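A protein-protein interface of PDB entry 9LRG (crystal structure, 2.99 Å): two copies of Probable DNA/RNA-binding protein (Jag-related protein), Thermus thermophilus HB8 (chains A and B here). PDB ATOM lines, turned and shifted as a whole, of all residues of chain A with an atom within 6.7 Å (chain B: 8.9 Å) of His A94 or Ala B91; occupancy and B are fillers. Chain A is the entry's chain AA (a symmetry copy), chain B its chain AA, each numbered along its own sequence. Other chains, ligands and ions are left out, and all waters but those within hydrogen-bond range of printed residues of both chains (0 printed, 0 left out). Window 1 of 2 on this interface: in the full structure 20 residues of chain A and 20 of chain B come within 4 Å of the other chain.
Among the printed residues, pairs that only touch across the chains: Ala A91 with His B94 (3.9 Å), Ala A91 with Leu B95 (3.7 Å), Val A92 with Leu B95 (3.6 Å), His A94 with Ala B91 (3.9 Å), His A94 with Glu B175 (3.7 Å), Leu A95 with Leu B50 (3.95 Å), Leu A95 with Ala B91 (3.7 Å), Leu A95 with Val B92 (3.6 Å), Leu A95 with Leu B95 (3.7 Å), Val A98 with Arg B87 (3.5 Å), Val A98 with Thr B88 (3.4 Å) and Val A99 with Leu B54 (3.8 Å).
Printed residues of chain B that touch a printed residue of chain A: Leu B50, Leu B54, Arg B87, Thr B88, Ala B91, Val B92, His B94, Leu B95 and Glu B175.
Hydrophobic or aromatic side chains of chain A that line the printed part of chain B: Ala A91, Val A92, His A94, Leu A95, Val A98 and Val A99.
Among the printed residues, 12 pairs touch across the chains.
Among the printed residues, no Asp or Glu carboxylate lies within 4 Å of a Lys or Arg side-chain nitrogen of the other chain.
Of chain B, only Ala B91 (3.9 Å) and Glu B175 (3.7 Å) come within 4 Å of His A94.
Of chain B, only Leu B50, Ala B91, Val B92 and Leu B95 come within 4 Å of Leu A95.
Of the printed residues of chain A, Thr B88 touches Val A98.
Ala B91 touches two residues of chain A.
Printed residues of chain A within 4 Å of Val B92: Leu A95 (3.6 Å).
The nearest residue of chain B that does not touch His A94 is Arg B87 (4.03 Å).
The nearest printed residue of chain A that does not touch His B94 is His A94 (5.2 Å).
Ala A91 touches His B94, and with the chains exchanged His A94 touches Ala B91.
Ala A91 touches Leu B95, and with the chains exchanged Leu A95 touches Ala B91.
Val A92 touches Leu B95, and with the chains exchanged Leu A95 touches Val B92.
Leu B95 touches its own counterpart, Leu A95.
11 positions are printed for both chains.
The backbone carbonyl oxygen (O) of Ile B82 is in hydrogen-bond range of the backbone NH (N) of Thr B88 (3.3 Å).
The guanidinium group (NH2) of Arg B87 is in salt-bridge range of the side-chain carboxylate (OE2) of Glu B175.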
ATOM      1  N   LEU A  89      29.446  11.327 -24.381  1.00  0.00           N
ATOM      2  CA  LEU A  89      29.588  10.189 -25.283  1.00  0.00           C
ATOM      3  C   LEU A  89      28.745   9.007 -24.818  1.00  0.00           C
ATOM      4  O   LEU A  89      28.122   8.323 -25.638  1.00  0.00           O
ATOM      5  CB  LEU A  89      31.062   9.795 -25.399  1.00  0.00           C
ATOM      6  CG  LEU A  89      31.435   8.687 -26.389  1.00  0.00           C
ATOM      7  CD1 LEU A  89      32.761   9.001 -27.060  1.00  0.00           C
ATOM      8  CD2 LEU A  89      31.507   7.331 -25.704  1.00  0.00           C
ATOM      9  N   ARG A  90      28.712   8.751 -23.508  1.00  0.00           N
ATOM     10  CA  ARG A  90      27.922   7.633 -23.006  1.00  0.00           C
ATOM     11  C   ARG A  90      26.428   7.923 -23.066  1.00  0.00           C
ATOM     12  O   ARG A  90      25.630   7.003 -23.269  1.00  0.00           O
ATOM     13  CB  ARG A  90      28.339   7.284 -21.578  1.00  0.00           C
ATOM     14  CG  ARG A  90      29.630   6.485 -21.491  1.00  0.00           C
ATOM     15  CD  ARG A  90      29.850   5.944 -20.088  1.00  0.00           C
ATOM     16  NE  ARG A  90      30.001   7.011 -19.107  1.00  0.00           N
ATOM     17  CZ  ARG A  90      31.161   7.565 -18.778  1.00  0.00           C
ATOM     18  NH1 ARG A  90      32.297   7.169 -19.332  1.00  0.00           N
ATOM     19  NH2 ARG A  90      31.182   8.538 -17.873  1.00  0.00           N
ATOM     20  N   ALA A  91      26.030   9.187 -22.891  1.00  0.00           N
ATOM     21  CA  ALA A  91      24.618   9.531 -23.015  1.00  0.00           C
ATOM     22  C   ALA A  91      24.135   9.354 -24.449  1.00  0.00           C
ATOM     23  O   ALA A  91      23.029   8.850 -24.680  1.00  0.00           O
ATOM     24  CB  ALA A  91      24.380  10.963 -22.538  1.00  0.00           C
ATOM     25  N   VAL A  92      24.949   9.760 -25.426  1.00  0.00           N
ATOM     26  CA  VAL A  92      24.611   9.508 -26.822  1.00  0.00           C
ATOM     27  C   VAL A  92      24.606   8.011 -27.105  1.00  0.00           C
ATOM     28  O   VAL A  92      23.706   7.492 -27.775  1.00  0.00           O
ATOM     29  CB  VAL A  92      25.584  10.255 -27.753  1.00  0.00           C
ATOM     30  CG1 VAL A  92      25.323   9.883 -29.203  1.00  0.00           C
ATOM     31  CG2 VAL A  92      25.465  11.757 -27.556  1.00  0.00           C
ATOM     32  N   GLU A  93      25.608   7.295 -26.588  1.00  0.00           N
ATOM     33  CA  GLU A  93      25.692   5.856 -26.813  1.00  0.00           C
ATOM     34  C   GLU A  93      24.509   5.126 -26.191  1.00  0.00           C
ATOM     35  O   GLU A  93      23.954   4.199 -26.794  1.00  0.00           O
ATOM     36  CB  GLU A  93      27.008   5.320 -26.249  1.00  0.00           C
ATOM     37  CG  GLU A  93      27.248   3.842 -26.514  1.00  0.00           C
ATOM     38  CD  GLU A  93      28.512   3.332 -25.851  1.00  0.00           C
ATOM     39  OE1 GLU A  93      28.658   3.515 -24.624  1.00  0.00           O
ATOM     40  OE2 GLU A  93      29.365   2.755 -26.561  1.00  0.00           O
ATOM     41  N   HIS A  94      24.107   5.532 -24.984  1.00  0.00           N
ATOM     42  CA  HIS A  94      23.019   4.843 -24.295  1.00  0.00           C
ATOM     43  C   HIS A  94      21.696   5.029 -25.028  1.00  0.00           C
ATOM     44  O   HIS A  94      20.941   4.068 -25.216  1.00  0.00           O
ATOM     45  CB  HIS A  94      22.913   5.340 -22.853  1.00  0.00           C
ATOM     46  CG  HIS A  94      21.742   4.781 -22.108  1.00  0.00           C
ATOM     47  ND1 HIS A  94      21.489   3.428 -22.026  1.00  0.00           N
ATOM     48  CD2 HIS A  94      20.755   5.390 -21.411  1.00  0.00           C
ATOM     49  CE1 HIS A  94      20.396   3.229 -21.311  1.00  0.00           C
ATOM     50  NE2 HIS A  94      19.931   4.404 -20.926  1.00  0.00           N
ATOM     51  N   LEU A  95      21.397   6.261 -25.448  1.00  0.00           N
ATOM     52  CA  LEU A  95      20.151   6.508 -26.168  1.00  0.00           C
ATOM     53  C   LEU A  95      20.114   5.740 -27.484  1.00  0.00           C
ATOM     54  O   LEU A  95      19.075   5.186 -27.857  1.00  0.00           O
ATOM     55  CB  LEU A  95      19.970   8.006 -26.416  1.00  0.00           C
ATOM     56  CG  LEU A  95      18.779   8.387 -27.298  1.00  0.00           C
ATOM     57  CD1 LEU A  95      17.484   7.830 -26.728  1.00  0.00           C
ATOM     58  CD2 LEU A  95      18.684   9.895 -27.473  1.00  0.00           C
ATOM     59  N   ALA A  96      21.241   5.692 -28.197  1.00  0.00           N
ATOM     60  CA  ALA A  96      21.287   4.929 -29.437  1.00  0.00           C
ATOM     61  C   ALA A  96      21.133   3.435 -29.185  1.00  0.00           C
ATOM     62  O   ALA A  96      20.561   2.725 -30.019  1.00  0.00           O
ATOM     63  CB  ALA A  96      22.590   5.218 -30.183  1.00  0.00           C
ATOM     64  N   ARG A  97      21.626   2.940 -28.047  1.00  0.00           N
ATOM     65  CA  ARG A  97      21.447   1.530 -27.716  1.00  0.00           C
ATOM     66  C   ARG A  97      19.988   1.212 -27.416  1.00  0.00           C
ATOM     67  O   ARG A  97      19.486   0.150 -27.804  1.00  0.00           O
ATOM     68  CB  ARG A  97      22.323   1.149 -26.523  1.00  0.00           C
ATOM     69  CG  ARG A  97      23.799   0.969 -26.835  1.00  0.00           C
ATOM     70  CD  ARG A  97      24.578   0.695 -25.556  1.00  0.00           C
ATOM     71  NE  ARG A  97      25.984   0.403 -25.811  1.00  0.00           N
ATOM     72  CZ  ARG A  97      26.894   0.231 -24.861  1.00  0.00           C
ATOM     73  NH1 ARG A  97      26.582   0.320 -23.579  1.00  0.00           N
ATOM     74  NH2 ARG A  97      28.151  -0.035 -25.210  1.00  0.00           N
ATOM     75  N   VAL A  98      19.294   2.116 -26.721  1.00  0.00           N
ATOM     76  CA  VAL A  98      17.906   1.864 -26.347  1.00  0.00           C
ATOM     77  C   VAL A  98      17.012   1.840 -27.581  1.00  0.00           C
ATOM     78  O   VAL A  98      16.154   0.961 -27.724  1.00  0.00           O
ATOM     79  CB  VAL A  98      17.431   2.910 -25.323  1.00  0.00           C
ATOM     80  CG1 VAL A  98      15.940   2.770 -25.068  1.00  0.00           C
ATOM     81  CG2 VAL A  98      18.207   2.767 -24.024  1.00  0.00           C
ATOM     82  N   VAL A  99      17.201   2.797 -28.491  1.00  0.00           N
ATOM     83  CA  VAL A  99      16.373   2.845 -29.691  1.00  0.00           C
ATOM     84  C   VAL A  99      16.712   1.687 -30.623  1.00  0.00           C
ATOM     85  O   VAL A  99      15.829   1.124 -31.282  1.00  0.00           O
ATOM     86  CB  VAL A  99      16.527   4.208 -30.391  1.00  0.00           C
ATOM     87  CG1 VAL A  99      15.582   4.308 -31.578  1.00  0.00           C
ATOM     88  CG2 VAL A  99      16.264   5.336 -29.409  1.00  0.00           C
ATOM     89  N   LEU A 110      26.035  -2.106 -29.395  1.00  0.00           N
ATOM     90  CA  LEU A 110      26.598  -0.905 -29.996  1.00  0.00           C
ATOM     91  C   LEU A 110      27.728  -0.363 -29.130  1.00  0.00           C
ATOM     92  O   LEU A 110      27.568  -0.210 -27.915  1.00  0.00           O
ATOM     93  CB  LEU A 110      25.520   0.163 -30.187  1.00  0.00           C
ATOM     94  CG  LEU A 110      26.007   1.551 -30.615  1.00  0.00           C
ATOM     95  CD1 LEU A 110      26.796   1.481 -31.912  1.00  0.00           C
ATOM     96  CD2 LEU A 110      24.830   2.493 -30.760  1.00  0.00           C
ATOM     97  N   LEU A 112      30.238   2.915 -29.042  1.00  0.00           N
ATOM     98  CA  LEU A 112      30.509   4.247 -29.563  1.00  0.00           C
ATOM     99  C   LEU A 112      31.876   4.722 -29.088  1.00  0.00           C
ATOM    100  O   LEU A 112      32.221   4.574 -27.912  1.00  0.00           O
ATOM    101  CB  LEU A 112      29.423   5.231 -29.123  1.00  0.00           C
ATOM    102  CG  LEU A 112      29.442   6.634 -29.734  1.00  0.00           C
ATOM    103  CD1 LEU A 112      29.246   6.572 -31.239  1.00  0.00           C
ATOM    104  CD2 LEU A 112      28.378   7.507 -29.092  1.00  0.00           C
ATOM    105  N   PHE B  46      17.375  21.456 -29.893  1.00  0.00           N
ATOM    106  CA  PHE B  46      18.015  20.151 -29.757  1.00  0.00           C
ATOM    107  C   PHE B  46      16.981  19.049 -29.554  1.00  0.00           C
ATOM    108  O   PHE B  46      16.932  18.079 -30.319  1.00  0.00           O
ATOM    109  CB  PHE B  46      19.016  20.170 -28.601  1.00  0.00           C
ATOM    110  CG  PHE B  46      19.657  18.836 -28.337  1.00  0.00           C
ATOM    111  CD1 PHE B  46      20.735  18.410 -29.094  1.00  0.00           C
ATOM    112  CD2 PHE B  46      19.179  18.007 -27.335  1.00  0.00           C
ATOM    113  CE1 PHE B  46      21.324  17.182 -28.857  1.00  0.00           C
ATOM    114  CE2 PHE B  46      19.763  16.777 -27.093  1.00  0.00           C
ATOM    115  CZ  PHE B  46      20.838  16.365 -27.854  1.00  0.00           C
ATOM    116  N   LEU B  47      16.153  19.175 -28.514  1.00  0.00           N
ATOM    117  CA  LEU B  47      15.131  18.163 -28.260  1.00  0.00           C
ATOM    118  C   LEU B  47      14.139  18.081 -29.412  1.00  0.00           C
ATOM    119  O   LEU B  47      13.691  16.988 -29.777  1.00  0.00           O
ATOM    120  CB  LEU B  47      14.405  18.461 -26.948  1.00  0.00           C
ATOM    121  CG  LEU B  47      14.634  17.493 -25.787  1.00  0.00           C
ATOM    122  CD1 LEU B  47      13.817  17.917 -24.576  1.00  0.00           C
ATOM    123  CD2 LEU B  47      14.284  16.076 -26.204  1.00  0.00           C
ATOM    124  N   LEU B  50      15.713  16.143 -32.039  1.00  0.00           N
ATOM    125  CA  LEU B  50      15.909  14.772 -31.582  1.00  0.00           C
ATOM    126  C   LEU B  50      14.597  13.996 -31.593  1.00  0.00           C
ATOM    127  O   LEU B  50      14.581  12.796 -31.892  1.00  0.00           O
ATOM    128  CB  LEU B  50      16.529  14.770 -30.184  1.00  0.00           C
ATOM    129  CG  LEU B  50      16.747  13.414 -29.510  1.00  0.00           C
ATOM    130  CD1 LEU B  50      17.512  12.472 -30.423  1.00  0.00           C
ATOM    131  CD2 LEU B  50      17.477  13.591 -28.187  1.00  0.00           C
ATOM    132  N   LEU B  54      13.082  10.391 -33.818  1.00  0.00           N
ATOM    133  CA  LEU B  54      12.322   9.282 -33.257  1.00  0.00           C
ATOM    134  C   LEU B  54      10.938   9.153 -33.881  1.00  0.00           C
ATOM    135  O   LEU B  54      10.457   8.033 -34.090  1.00  0.00           O
ATOM    136  CB  LEU B  54      12.191   9.451 -31.740  1.00  0.00           C
ATOM    137  CG  LEU B  54      13.481   9.342 -30.928  1.00  0.00           C
ATOM    138  CD1 LEU B  54      13.254   9.823 -29.506  1.00  0.00           C
ATOM    139  CD2 LEU B  54      13.987   7.910 -30.934  1.00  0.00           C
ATOM    140  N   PHE B  81       7.717   6.304 -27.634  1.00  0.00           N
ATOM    141  CA  PHE B  81       8.642   7.301 -27.103  1.00  0.00           C
ATOM    142  C   PHE B  81       8.921   7.066 -25.624  1.00  0.00           C
ATOM    143  O   PHE B  81      10.046   7.282 -25.157  1.00  0.00           O
ATOM    144  CB  PHE B  81       8.091   8.708 -27.324  1.00  0.00           C
ATOM    145  CG  PHE B  81       8.779   9.760 -26.503  1.00  0.00           C
ATOM    146  CD1 PHE B  81      10.054  10.192 -26.831  1.00  0.00           C
ATOM    147  CD2 PHE B  81       8.153  10.316 -25.400  1.00  0.00           C
ATOM    148  CE1 PHE B  81      10.691  11.156 -26.074  1.00  0.00           C
ATOM    149  CE2 PHE B  81       8.784  11.281 -24.639  1.00  0.00           C
ATOM    150  CZ  PHE B  81      10.054  11.702 -24.977  1.00  0.00           C
ATOM    151  N   ILE B  82       7.909   6.638 -24.867  1.00  0.00           N
ATOM    152  CA  ILE B  82       8.135   6.294 -23.467  1.00  0.00           C
ATOM    153  C   ILE B  82       9.035   5.070 -23.363  1.00  0.00           C
ATOM    154  O   ILE B  82       9.985   5.046 -22.571  1.00  0.00           O
ATOM    155  CB  ILE B  82       6.794   6.080 -22.744  1.00  0.00           C
ATOM    156  CG1 ILE B  82       6.006   7.390 -22.679  1.00  0.00           C
ATOM    157  CG2 ILE B  82       7.020   5.523 -21.345  1.00  0.00           C
ATOM    158  CD1 ILE B  82       4.644   7.254 -22.038  1.00  0.00           C
ATOM    159  N   GLY B  83       8.765   4.046 -24.167  1.00  0.00           N
ATOM    160  CA  GLY B  83       9.579   2.850 -24.164  1.00  0.00           C
ATOM    161  C   GLY B  83       9.241   1.923 -23.014  1.00  0.00           C
ATOM    162  O   GLY B  83       8.336   2.162 -22.212  1.00  0.00           O
ATOM    163  N   LYS B  84       9.997   0.832 -22.940  1.00  0.00           N
ATOM    164  CA  LYS B  84       9.781  -0.165 -21.900  1.00  0.00           C
ATOM    165  C   LYS B  84      10.187   0.401 -20.545  1.00  0.00           C
ATOM    166  O   LYS B  84      11.360   0.723 -20.326  1.00  0.00           O
ATOM    167  CB  LYS B  84      10.570  -1.433 -22.213  1.00  0.00           C
ATOM    168  N   GLU B  85       9.213   0.531 -19.643  1.00  0.00           N
ATOM    169  CA  GLU B  85       9.415   1.044 -18.289  1.00  0.00           C
ATOM    170  C   GLU B  85       9.984   2.459 -18.279  1.00  0.00           C
ATOM    171  O   GLU B  85      10.608   2.874 -17.298  1.00  0.00           O
ATOM    172  CB  GLU B  85      10.314   0.111 -17.468  1.00  0.00           C
ATOM    173  CG  GLU B  85       9.895  -1.348 -17.512  1.00  0.00           C
ATOM    174  CD  GLU B  85       8.493  -1.571 -16.982  1.00  0.00           C
ATOM    175  OE1 GLU B  85       8.090  -0.857 -16.040  1.00  0.00           O
ATOM    176  OE2 GLU B  85       7.790  -2.459 -17.512  1.00  0.00           O
ATOM    177  N   GLY B  86       9.777   3.214 -19.355  1.00  0.00           N
ATOM    178  CA  GLY B  86      10.291   4.566 -19.424  1.00  0.00           C
ATOM    179  C   GLY B  86      11.764   4.680 -19.739  1.00  0.00           C
ATOM    180  O   GLY B  86      12.345   5.750 -19.537  1.00  0.00           O
ATOM    181  N   ARG B  87      12.391   3.608 -20.232  1.00  0.00           N
ATOM    182  CA  ARG B  87      13.816   3.666 -20.544  1.00  0.00           C
ATOM    183  C   ARG B  87      14.093   4.607 -21.710  1.00  0.00           C
ATOM    184  O   ARG B  87      15.073   5.361 -21.687  1.00  0.00           O
ATOM    185  CB  ARG B  87      14.349   2.266 -20.846  1.00  0.00           C
ATOM    186  CG  ARG B  87      14.433   1.358 -19.630  1.00  0.00           C
ATOM    187  CD  ARG B  87      15.000  -0.012 -19.980  1.00  0.00           C
ATOM    188  NE  ARG B  87      16.394   0.053 -20.405  1.00  0.00           N
ATOM    189  CZ  ARG B  87      16.810  -0.113 -21.654  1.00  0.00           C
ATOM    190  NH1 ARG B  87      15.961  -0.369 -22.636  1.00  0.00           N
ATOM    191  NH2 ARG B  87      18.110  -0.027 -21.922  1.00  0.00           N
ATOM    192  N   THR B  88      13.243   4.578 -22.740  1.00  0.00           N
ATOM    193  CA  THR B  88      13.440   5.470 -23.878  1.00  0.00           C
ATOM    194  C   THR B  88      13.232   6.926 -23.478  1.00  0.00           C
ATOM    195  O   THR B  88      14.003   7.803 -23.883  1.00  0.00           O
ATOM    196  CB  THR B  88      12.497   5.085 -25.019  1.00  0.00           C
ATOM    197  OG1 THR B  88      12.688   3.704 -25.352  1.00  0.00           O
ATOM    198  CG2 THR B  88      12.771   5.936 -26.250  1.00  0.00           C
ATOM    199  N   LEU B  89      12.200   7.199 -22.674  1.00  0.00           N
ATOM    200  CA  LEU B  89      11.959   8.565 -22.221  1.00  0.00           C
ATOM    201  C   LEU B  89      13.098   9.064 -21.339  1.00  0.00           C
ATOM    202  O   LEU B  89      13.515  10.222 -21.454  1.00  0.00           O
ATOM    203  CB  LEU B  89      10.623   8.641 -21.477  1.00  0.00           C
ATOM    204  CG  LEU B  89      10.133  10.017 -21.017  1.00  0.00           C
ATOM    205  CD1 LEU B  89       8.625  10.122 -21.170  1.00  0.00           C
ATOM    206  CD2 LEU B  89      10.530  10.295 -19.575  1.00  0.00           C
ATOM    207  N   ARG B  90      13.616   8.207 -20.456  1.00  0.00           N
ATOM    208  CA  ARG B  90      14.707   8.629 -19.587  1.00  0.00           C
ATOM    209  C   ARG B  90      16.020   8.756 -20.348  1.00  0.00           C
ATOM    210  O   ARG B  90      16.848   9.607 -20.010  1.00  0.00           O
ATOM    211  CB  ARG B  90      14.864   7.659 -18.416  1.00  0.00           C
ATOM    212  CG  ARG B  90      13.835   7.854 -17.314  1.00  0.00           C
ATOM    213  CD  ARG B  90      14.198   7.054 -16.073  1.00  0.00           C
ATOM    214  NE  ARG B  90      14.206   5.619 -16.331  1.00  0.00           N
ATOM    215  CZ  ARG B  90      13.149   4.830 -16.195  1.00  0.00           C
ATOM    216  NH1 ARG B  90      11.978   5.305 -15.797  1.00  0.00           N
ATOM    217  NH2 ARG B  90      13.268   3.533 -16.462  1.00  0.00           N
ATOM    218  N   ALA B  91      16.231   7.923 -21.371  1.00  0.00           N
ATOM    219  CA  ALA B  91      17.437   8.052 -22.182  1.00  0.00           C
ATOM    220  C   ALA B  91      17.430   9.358 -22.969  1.00  0.00           C
ATOM    221  O   ALA B  91      18.462  10.031 -23.073  1.00  0.00           O
ATOM    222  CB  ALA B  91      17.574   6.855 -23.122  1.00  0.00           C
ATOM    223  N   VAL B  92      16.278   9.731 -23.528  1.00  0.00           N
ATOM    224  CA  VAL B  92      16.162  11.027 -24.189  1.00  0.00           C
ATOM    225  C   VAL B  92      16.328  12.153 -23.177  1.00  0.00           C
ATOM    226  O   VAL B  92      17.023  13.143 -23.434  1.00  0.00           O
ATOM    227  CB  VAL B  92      14.819  11.131 -24.935  1.00  0.00           C
ATOM    228  CG1 VAL B  92      14.635  12.527 -25.505  1.00  0.00           C
ATOM    229  CG2 VAL B  92      14.739  10.088 -26.038  1.00  0.00           C
ATOM    230  N   GLU B  93      15.697  12.013 -22.008  1.00  0.00           N
ATOM    231  CA  GLU B  93      15.790  13.046 -20.981  1.00  0.00           C
ATOM    232  C   GLU B  93      17.221  13.207 -20.482  1.00  0.00           C
ATOM    233  O   GLU B  93      17.689  14.332 -20.270  1.00  0.00           O
ATOM    234  CB  GLU B  93      14.855  12.707 -19.821  1.00  0.00           C
ATOM    235  CG  GLU B  93      14.797  13.766 -18.732  1.00  0.00           C
ATOM    236  CD  GLU B  93      13.937  13.344 -17.556  1.00  0.00           C
ATOM    237  OE1 GLU B  93      14.185  12.255 -16.997  1.00  0.00           O
ATOM    238  OE2 GLU B  93      13.008  14.098 -17.196  1.00  0.00           O
ATOM    239  N   HIS B  94      17.930  12.093 -20.293  1.00  0.00           N
ATOM    240  CA  HIS B  94      19.288  12.160 -19.759  1.00  0.00           C
ATOM    241  C   HIS B  94      20.233  12.844 -20.739  1.00  0.00           C
ATOM    242  O   HIS B  94      21.033  13.702 -20.347  1.00  0.00           O
ATOM    243  CB  HIS B  94      19.788  10.757 -19.415  1.00  0.00           C
ATOM    244  CG  HIS B  94      21.219  10.718 -18.979  1.00  0.00           C
ATOM    245  ND1 HIS B  94      21.712  11.516 -17.970  1.00  0.00           N
ATOM    246  CD2 HIS B  94      22.263   9.976 -19.417  1.00  0.00           C
ATOM    247  CE1 HIS B  94      23.000  11.268 -17.805  1.00  0.00           C
ATOM    248  NE2 HIS B  94      23.359  10.338 -18.671  1.00  0.00           N
ATOM    249  N   LEU B  95      20.157  12.476 -22.020  1.00  0.00           N
ATOM    250  CA  LEU B  95      21.025  13.099 -23.016  1.00  0.00           C
ATOM    251  C   LEU B  95      20.747  14.592 -23.131  1.00  0.00           C
ATOM    252  O   LEU B  95      21.677  15.397 -23.249  1.00  0.00           O
ATOM    253  CB  LEU B  95      20.852  12.415 -24.373  1.00  0.00           C
ATOM    254  CG  LEU B  95      21.591  13.075 -25.539  1.00  0.00           C
ATOM    255  CD1 LEU B  95      23.078  13.190 -25.241  1.00  0.00           C
ATOM    256  CD2 LEU B  95      21.361  12.314 -26.835  1.00  0.00           C
ATOM    257  N   ALA B  96      19.471  14.983 -23.091  1.00  0.00           N
ATOM    258  CA  ALA B  96      19.140  16.402 -23.142  1.00  0.00           C
ATOM    259  C   ALA B  96      19.624  17.136 -21.898  1.00  0.00           C
ATOM    260  O   ALA B  96      19.993  18.313 -21.982  1.00  0.00           O
ATOM    261  CB  ALA B  96      17.633  16.582 -23.322  1.00  0.00           C
ATOM    262  N   ARG B  97      19.637  16.467 -20.743  1.00  0.00           N
ATOM    263  CA  ARG B  97      20.156  17.094 -19.532  1.00  0.00           C
ATOM    264  C   ARG B  97      21.662  17.304 -19.618  1.00  0.00           C
ATOM    265  O   ARG B  97      22.178  18.334 -19.168  1.00  0.00           O
ATOM    266  CB  ARG B  97      19.813  16.248 -18.307  1.00  0.00           C
ATOM    267  CG  ARG B  97      18.373  16.347 -17.833  1.00  0.00           C
ATOM    268  CD  ARG B  97      18.130  15.386 -16.679  1.00  0.00           C
ATOM    269  NE  ARG B  97      16.793  15.519 -16.113  1.00  0.00           N
ATOM    270  CZ  ARG B  97      16.301  14.730 -15.167  1.00  0.00           C
ATOM    271  NH1 ARG B  97      17.008  13.733 -14.660  1.00  0.00           N
ATOM    272  NH2 ARG B  97      15.066  14.946 -14.721  1.00  0.00           N
ATOM    273  N   VAL B  98      22.384  16.336 -20.185  1.00  0.00           N
ATOM    274  CA  VAL B  98      23.839  16.436 -20.260  1.00  0.00           C
ATOM    275  C   VAL B  98      24.253  17.562 -21.198  1.00  0.00           C
ATOM    276  O   VAL B  98      25.150  18.353 -20.881  1.00  0.00           O
ATOM    277  CB  VAL B  98      24.444  15.087 -20.688  1.00  0.00           C
ATOM    278  CG1 VAL B  98      25.935  15.229 -20.948  1.00  0.00           C
ATOM    279  CG2 VAL B  98      24.189  14.032 -19.626  1.00  0.00           C
ATOM    280  N   LEU B 112      11.335  15.780 -18.344  1.00  0.00           N
ATOM    281  CA  LEU B 112      10.679  15.333 -19.565  1.00  0.00           C
ATOM    282  C   LEU B 112       9.493  14.441 -19.220  1.00  0.00           C
ATOM    283  O   LEU B 112       9.596  13.556 -18.364  1.00  0.00           O
ATOM    284  CB  LEU B 112      11.664  14.580 -20.463  1.00  0.00           C
ATOM    285  CG  LEU B 112      11.200  14.202 -21.871  1.00  0.00           C
ATOM    286  CD1 LEU B 112      10.884  15.443 -22.688  1.00  0.00           C
ATOM    287  CD2 LEU B 112      12.252  13.357 -22.568  1.00  0.00           C
ATOM    288  N   GLY B 174      24.041  -0.690 -12.348  1.00  0.00           N
ATOM    289  CA  GLY B 174      23.622  -0.144 -13.631  1.00  0.00           C
ATOM    290  C   GLY B 174      22.135  -0.328 -13.855  1.00  0.00           C
ATOM    291  O   GLY B 174      21.309  -0.054 -12.977  1.00  0.00           O
ATOM    292  N   GLU B 175      21.784  -0.802 -15.052  1.00  0.00           N
ATOM    293  CA  GLU B 175      20.389  -1.035 -15.399  1.00  0.00           C
ATOM    294  C   GLU B 175      19.776  -2.204 -14.640  1.00  0.00           C
ATOM    295  O   GLU B 175      18.560  -2.402 -14.724  1.00  0.00           O
ATOM    296  CB  GLU B 175      20.260  -1.267 -16.904  1.00  0.00           C
ATOM    297  CG  GLU B 175      20.364   0.004 -17.729  1.00  0.00           C
ATOM    298  CD  GLU B 175      20.788  -0.263 -19.159  1.00  0.00           C
ATOM    299  OE1 GLU B 175      21.990  -0.521 -19.385  1.00  0.00           O
ATOM    300  OE2 GLU B 175      19.919  -0.223 -20.057  1.00  0.00           O
